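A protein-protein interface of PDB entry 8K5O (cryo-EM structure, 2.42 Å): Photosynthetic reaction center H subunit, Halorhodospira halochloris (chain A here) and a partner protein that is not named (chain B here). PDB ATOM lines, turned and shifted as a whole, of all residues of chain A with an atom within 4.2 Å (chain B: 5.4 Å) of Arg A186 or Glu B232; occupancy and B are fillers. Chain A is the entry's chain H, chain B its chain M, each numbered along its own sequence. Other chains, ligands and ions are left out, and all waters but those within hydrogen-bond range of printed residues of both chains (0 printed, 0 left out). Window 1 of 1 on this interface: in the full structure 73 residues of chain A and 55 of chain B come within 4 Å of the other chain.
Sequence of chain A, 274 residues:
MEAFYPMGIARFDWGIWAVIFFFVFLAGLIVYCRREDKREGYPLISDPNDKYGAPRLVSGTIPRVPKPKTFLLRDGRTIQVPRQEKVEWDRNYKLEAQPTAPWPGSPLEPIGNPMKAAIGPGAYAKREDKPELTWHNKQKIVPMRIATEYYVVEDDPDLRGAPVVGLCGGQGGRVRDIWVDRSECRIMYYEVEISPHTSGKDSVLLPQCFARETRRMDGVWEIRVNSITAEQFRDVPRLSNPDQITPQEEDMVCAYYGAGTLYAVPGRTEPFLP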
ATOM      1  N   VAL A 180      25.555  -3.771  27.433  1.00  0.00           N
ATOM      2  CA  VAL A 180      24.255  -3.873  28.077  1.00  0.00           C
ATOM      3  C   VAL A 180      23.183  -3.982  27.007  1.00  0.00           C
ATOM      4  O   VAL A 180      23.345  -3.513  25.875  1.00  0.00           O
ATOM      5  CB  VAL A 180      23.972  -2.671  29.003  1.00  0.00           C
ATOM      6  CG1 VAL A 180      25.006  -2.596  30.105  1.00  0.00           C
ATOM      7  CG2 VAL A 180      23.944  -1.383  28.207  1.00  0.00           C
ATOM      8  N   ASP A 181      22.078  -4.614  27.378  1.00  0.00           N
ATOM      9  CA  ASP A 181      20.887  -4.645  26.546  1.00  0.00           C
ATOM     10  C   ASP A 181      20.009  -3.460  26.928  1.00  0.00           C
ATOM     11  O   ASP A 181      19.604  -3.330  28.087  1.00  0.00           O
ATOM     12  CB  ASP A 181      20.145  -5.967  26.721  1.00  0.00           C
ATOM     13  CG  ASP A 181      19.006  -6.132  25.745  1.00  0.00           C
ATOM     14  OD1 ASP A 181      18.663  -5.161  25.050  1.00  0.00           O
ATOM     15  OD2 ASP A 181      18.467  -7.249  25.650  1.00  0.00           O
ATOM     16  N   GLU A 184      16.466  -4.829  27.892  1.00  0.00           N
ATOM     17  CA  GLU A 184      16.438  -5.659  29.087  1.00  0.00           C
ATOM     18  C   GLU A 184      17.063  -4.986  30.300  1.00  0.00           C
ATOM     19  O   GLU A 184      16.839  -5.449  31.422  1.00  0.00           O
ATOM     20  CB  GLU A 184      17.163  -6.982  28.827  1.00  0.00           C
ATOM     21  CG  GLU A 184      16.439  -7.920  27.884  1.00  0.00           C
ATOM     22  CD  GLU A 184      15.160  -8.481  28.463  1.00  0.00           C
ATOM     23  OE1 GLU A 184      15.053  -8.595  29.702  1.00  0.00           O
ATOM     24  OE2 GLU A 184      14.266  -8.837  27.671  1.00  0.00           O
ATOM     25  N   CYS A 185      17.824  -3.910  30.101  1.00  0.00           N
ATOM     26  CA  CYS A 185      18.525  -3.218  31.182  1.00  0.00           C
ATOM     27  C   CYS A 185      19.390  -4.185  31.987  1.00  0.00           C
ATOM     28  O   CYS A 185      19.446  -4.131  33.217  1.00  0.00           O
ATOM     29  CB  CYS A 185      17.545  -2.472  32.089  1.00  0.00           C
ATOM     30  SG  CYS A 185      17.063  -0.841  31.482  1.00  0.00           S
ATOM     31  N   ARG A 186      20.069  -5.082  31.283  1.00  0.00           N
ATOM     32  CA  ARG A 186      20.972  -6.041  31.897  1.00  0.00           C
ATOM     33  C   ARG A 186      22.310  -6.005  31.180  1.00  0.00           C
ATOM     34  O   ARG A 186      22.400  -5.595  30.023  1.00  0.00           O
ATOM     35  CB  ARG A 186      20.422  -7.471  31.844  1.00  0.00           C
ATOM     36  CG  ARG A 186      19.203  -7.710  32.698  1.00  0.00           C
ATOM     37  CD  ARG A 186      18.923  -9.191  32.836  1.00  0.00           C
ATOM     38  NE  ARG A 186      18.699  -9.829  31.546  1.00  0.00           N
ATOM     39  CZ  ARG A 186      17.523  -9.898  30.939  1.00  0.00           C
ATOM     40  NH1 ARG A 186      16.435  -9.374  31.478  1.00  0.00           N
ATOM     41  NH2 ARG A 186      17.439 -10.500  29.759  1.00  0.00           N
ATOM     42  N   ILE A 187      23.349  -6.442  31.885  1.00  0.00           N
ATOM     43  CA  ILE A 187      24.642  -6.667  31.253  1.00  0.00           C
ATOM     44  C   ILE A 187      24.528  -7.891  30.358  1.00  0.00           C
ATOM     45  O   ILE A 187      24.184  -8.985  30.820  1.00  0.00           O
ATOM     46  CB  ILE A 187      25.743  -6.853  32.305  1.00  0.00           C
ATOM     47  CG1 ILE A 187      25.861  -5.604  33.174  1.00  0.00           C
ATOM     48  CG2 ILE A 187      27.073  -7.184  31.640  1.00  0.00           C
ATOM     49  CD1 ILE A 187      27.071  -5.581  34.057  1.00  0.00           C
ATOM     50  N   MET A 188      24.799  -7.710  29.070  1.00  0.00           N
ATOM     51  CA  MET A 188      24.834  -8.840  28.152  1.00  0.00           C
ATOM     52  C   MET A 188      26.236  -9.414  28.029  1.00  0.00           C
ATOM     53  O   MET A 188      26.426 -10.630  28.122  1.00  0.00           O
ATOM     54  CB  MET A 188      24.318  -8.427  26.773  1.00  0.00           C
ATOM     55  CG  MET A 188      22.828  -8.189  26.704  1.00  0.00           C
ATOM     56  SD  MET A 188      21.867  -9.678  27.019  1.00  0.00           S
ATOM     57  CE  MET A 188      21.254  -9.358  28.667  1.00  0.00           C
ATOM     58  N   ASN B   6      22.961 -17.941  37.063  1.00  0.00           N
ATOM     59  CA  ASN B   6      21.892 -17.095  36.531  1.00  0.00           C
ATOM     60  C   ASN B   6      20.734 -16.963  37.515  1.00  0.00           C
ATOM     61  O   ASN B   6      19.586 -16.763  37.117  1.00  0.00           O
ATOM     62  CB  ASN B   6      21.396 -17.610  35.176  1.00  0.00           C
ATOM     63  CG  ASN B   6      20.975 -16.495  34.244  1.00  0.00           C
ATOM     64  OD1 ASN B   6      21.142 -15.318  34.552  1.00  0.00           O
ATOM     65  ND2 ASN B   6      20.431 -16.862  33.093  1.00  0.00           N
ATOM     66  N   THR B   9      21.273 -11.324  39.646  1.00  0.00           N
ATOM     67  CA  THR B   9      22.070 -10.387  38.859  1.00  0.00           C
ATOM     68  C   THR B   9      23.062  -9.732  39.805  1.00  0.00           C
ATOM     69  O   THR B   9      22.707  -8.832  40.572  1.00  0.00           O
ATOM     70  CB  THR B   9      21.181  -9.358  38.173  1.00  0.00           C
ATOM     71  OG1 THR B   9      20.319 -10.016  37.239  1.00  0.00           O
ATOM     72  CG2 THR B   9      22.022  -8.330  37.441  1.00  0.00           C
ATOM     73  N   VAL B  13      22.842  -2.816  35.984  1.00  0.00           N
ATOM     74  CA  VAL B  13      23.075  -1.582  35.247  1.00  0.00           C
ATOM     75  C   VAL B  13      21.763  -0.820  35.156  1.00  0.00           C
ATOM     76  O   VAL B  13      20.696  -1.415  34.967  1.00  0.00           O
ATOM     77  CB  VAL B  13      23.663  -1.838  33.845  1.00  0.00           C
ATOM     78  CG1 VAL B  13      25.097  -2.304  33.960  1.00  0.00           C
ATOM     79  CG2 VAL B  13      22.828  -2.856  33.093  1.00  0.00           C
ATOM     80  N   ASP B  45      13.968  -6.958  36.586  1.00  0.00           N
ATOM     81  CA  ASP B  45      14.096  -5.523  36.384  1.00  0.00           C
ATOM     82  C   ASP B  45      13.981  -4.786  37.708  1.00  0.00           C
ATOM     83  O   ASP B  45      13.118  -5.087  38.535  1.00  0.00           O
ATOM     84  CB  ASP B  45      13.034  -5.012  35.416  1.00  0.00           C
ATOM     85  CG  ASP B  45      13.186  -5.583  34.029  1.00  0.00           C
ATOM     86  OD1 ASP B  45      14.330  -5.871  33.625  1.00  0.00           O
ATOM     87  OD2 ASP B  45      12.161  -5.732  33.336  1.00  0.00           O
ATOM     88  N   ILE B 223      15.708 -21.923  30.846  1.00  0.00           N
ATOM     89  CA  ILE B 223      16.102 -20.590  30.421  1.00  0.00           C
ATOM     90  C   ILE B 223      17.313 -20.110  31.203  1.00  0.00           C
ATOM     91  O   ILE B 223      18.202 -19.465  30.648  1.00  0.00           O
ATOM     92  CB  ILE B 223      14.909 -19.631  30.542  1.00  0.00           C
ATOM     93  CG1 ILE B 223      13.838 -20.018  29.525  1.00  0.00           C
ATOM     94  CG2 ILE B 223      15.349 -18.208  30.324  1.00  0.00           C
ATOM     95  CD1 ILE B 223      14.388 -20.436  28.188  1.00  0.00           C
ATOM     96  N   THR B 226      20.280 -22.044  29.754  1.00  0.00           N
ATOM     97  CA  THR B 226      20.632 -21.607  28.415  1.00  0.00           C
ATOM     98  C   THR B 226      20.831 -20.102  28.323  1.00  0.00           C
ATOM     99  O   THR B 226      21.053 -19.586  27.225  1.00  0.00           O
ATOM    100  CB  THR B 226      19.557 -22.060  27.423  1.00  0.00           C
ATOM    101  OG1 THR B 226      18.264 -21.785  27.967  1.00  0.00           O
ATOM    102  CG2 THR B 226      19.667 -23.541  27.168  1.00  0.00           C
ATOM    103  N   GLY B 227      20.745 -19.386  29.446  1.00  0.00           N
ATOM    104  CA  GLY B 227      21.066 -17.972  29.467  1.00  0.00           C
ATOM    105  C   GLY B 227      22.496 -17.683  29.092  1.00  0.00           C
ATOM    106  O   GLY B 227      22.824 -16.544  28.744  1.00  0.00           O
ATOM    107  N   ARG B 228      23.356 -18.698  29.147  1.00  0.00           N
ATOM    108  CA  ARG B 228      24.674 -18.603  28.547  1.00  0.00           C
ATOM    109  C   ARG B 228      24.596 -18.264  27.068  1.00  0.00           C
ATOM    110  O   ARG B 228      25.547 -17.707  26.517  1.00  0.00           O
ATOM    111  CB  ARG B 228      25.412 -19.922  28.734  1.00  0.00           C
ATOM    112  CG  ARG B 228      25.350 -20.484  30.126  1.00  0.00           C
ATOM    113  CD  ARG B 228      25.868 -21.901  30.150  1.00  0.00           C
ATOM    114  NE  ARG B 228      26.022 -22.395  31.510  1.00  0.00           N
ATOM    115  CZ  ARG B 228      26.832 -23.383  31.858  1.00  0.00           C
ATOM    116  NH1 ARG B 228      27.582 -24.006  30.966  1.00  0.00           N
ATOM    117  NH2 ARG B 228      26.885 -23.758  33.131  1.00  0.00           N
ATOM    118  N   ASN B 230      21.891 -16.502  25.659  1.00  0.00           N
ATOM    119  CA  ASN B 230      20.904 -15.435  25.508  1.00  0.00           C
ATOM    120  C   ASN B 230      19.505 -15.986  25.254  1.00  0.00           C
ATOM    121  O   ASN B 230      18.721 -15.414  24.496  1.00  0.00           O
ATOM    122  CB  ASN B 230      21.313 -14.465  24.400  1.00  0.00           C
ATOM    123  CG  ASN B 230      22.792 -14.163  24.412  1.00  0.00           C
ATOM    124  OD1 ASN B 230      23.475 -14.307  23.400  1.00  0.00           O
ATOM    125  ND2 ASN B 230      23.298 -13.745  25.562  1.00  0.00           N
ATOM    126  N   SER B 231      19.184 -17.101  25.903  1.00  0.00           N
ATOM    127  CA  SER B 231      17.876 -17.710  25.726  1.00  0.00           C
ATOM    128  C   SER B 231      16.784 -16.998  26.508  1.00  0.00           C
ATOM    129  O   SER B 231      15.602 -17.213  26.223  1.00  0.00           O
ATOM    130  CB  SER B 231      17.922 -19.178  26.139  1.00  0.00           C
ATOM    131  OG  SER B 231      17.805 -19.307  27.544  1.00  0.00           O
ATOM    132  N   GLU B 232      17.146 -16.169  27.489  1.00  0.00           N
ATOM    133  CA  GLU B 232      16.131 -15.452  28.252  1.00  0.00           C
ATOM    134  C   GLU B 232      15.455 -14.390  27.403  1.00  0.00           C
ATOM    135  O   GLU B 232      14.289 -14.060  27.637  1.00  0.00           O
ATOM    136  CB  GLU B 232      16.743 -14.837  29.512  1.00  0.00           C
ATOM    137  CG  GLU B 232      17.601 -13.616  29.269  1.00  0.00           C
ATOM    138  CD  GLU B 232      18.982 -13.964  28.759  1.00  0.00           C
ATOM    139  OE1 GLU B 232      19.458 -15.081  29.049  1.00  0.00           O
ATOM    140  OE2 GLU B 232      19.587 -13.121  28.063  1.00  0.00           O
ATOM    141  N   ARG B 233      16.162 -13.853  26.411  1.00  0.00           N
ATOM    142  CA  ARG B 233      15.549 -13.006  25.395  1.00  0.00           C
ATOM    143  C   ARG B 233      14.808 -13.926  24.433  1.00  0.00           C
ATOM    144  O   ARG B 233      15.267 -14.244  23.334  1.00  0.00           O
ATOM    145  CB  ARG B 233      16.597 -12.158  24.696  1.00  0.00           C
ATOM    146  CG  ARG B 233      17.236 -11.131  25.599  1.00  0.00           C
ATOM    147  CD  ARG B 233      18.252 -10.322  24.836  1.00  0.00           C
ATOM    148  NE  ARG B 233      19.448 -11.084  24.508  1.00  0.00           N
ATOM    149  CZ  ARG B 233      20.363 -10.679  23.639  1.00  0.00           C
ATOM    150  NH1 ARG B 233      20.200  -9.574  22.936  1.00  0.00           N
ATOM    151  NH2 ARG B 233      21.461 -11.403  23.467  1.00  0.00           N
ATOM    152  N   GLU B 234      13.633 -14.368  24.878  1.00  0.00           N
ATOM    153  CA  GLU B 234      12.903 -15.421  24.188  1.00  0.00           C
ATOM    154  C   GLU B 234      12.196 -14.933  22.937  1.00  0.00           C
ATOM    155  O   GLU B 234      11.961 -15.726  22.027  1.00  0.00           O
ATOM    156  CB  GLU B 234      11.895 -16.060  25.133  1.00  0.00           C
ATOM    157  CG  GLU B 234      12.500 -16.457  26.444  1.00  0.00           C
ATOM    158  CD  GLU B 234      11.505 -17.105  27.347  1.00  0.00           C
ATOM    159  OE1 GLU B 234      10.353 -16.636  27.379  1.00  0.00           O
ATOM    160  OE2 GLU B 234      11.872 -18.081  28.017  1.00  0.00           O
ATOM    161  N   ILE B 235      11.834 -13.653  22.874  1.00  0.00           N
ATOM    162  CA  ILE B 235      11.184 -13.137  21.675  1.00  0.00           C
ATOM    163  C   ILE B 235      12.119 -13.258  20.482  1.00  0.00           C
ATOM    164  O   ILE B 235      11.719 -13.689  19.393  1.00  0.00           O
ATOM    165  CB  ILE B 235      10.730 -11.683  21.899  1.00  0.00           C
ATOM    166  CG1 ILE B 235       9.860 -11.588  23.155  1.00  0.00           C
ATOM    167  CG2 ILE B 235       9.997 -11.163  20.681  1.00  0.00           C
ATOM    168  CD1 ILE B 235       8.803 -12.681  23.271  1.00  0.00           C
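OE2 of Glu B232 lies within salt-bridge range of NH2 of Arg A186. The side-chain carboxylate (OD2) of Asp A181 lies within salt-bridge range of the guanidinium group (NH1) of Arg B233 (3.97 Å). The side-chain sulfur (SD) of Met A188 sits at hydrogen-bond distance from the guanidinium group (NE) of Arg B233, at 3.8 Å. OD1 of Asp B45 lies close to O of Glu A184. O of Val B13 lies close to O of Cys A185, at 3.5 Å.
The backbone NH (N) of Asp A181 is in hydrogen-bond range of the backbone carbonyl oxygen (O) of Arg A186. The side-chain carboxylate of Glu A184 lies within salt-bridge range of the guanidinium group of Arg A186 (3.1 Å).
Printed residues of chain B within 4 Å of Arg A186: Val B13 and Glu B232. Glu B232 touches one residue of chain A. Printed residues of chain B within 4 Å of Cys A185: Val B13. Of the printed residues of chain B, Met A188 touches Arg B233 (3.8 Å). Of the printed residues of chain B, Ile A187 touches Val B13. Printed residues of chain A within 4 Å of Asp B45: Glu A184. The nearest printed residue of chain A that does not touch Val B13 is Asp A181 (6.0 Å).
Among the printed residues, pairs that only touch across the chains: Ile A187 with Val B13 (3.5 Å), Val A180 with Val B13 (3.7 Å) and Arg A186 with Val B13 (3.7 Å).
Of the 14 printed residues of chain B, 4 touch a printed residue of chain A. Hydrophobic or aromatic side chains of chain B that line the printed part of chain A: Val B13. Along chain B the printed residues that touch a printed residue of chain A span positions 13 to 233. Of the 7 printed residues of chain A, 7 touch a printed residue of chain B. Among the printed residues, 8 pairs touch across the chains. Among the printed residues, Asp or Glu carboxylates within 4 Å of a Lys or Arg side-chain nitrogen of the other chain: Asp A181 with Arg B233 (3.97 Å) and Arg A186 with Glu B232 (3.8 Å).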
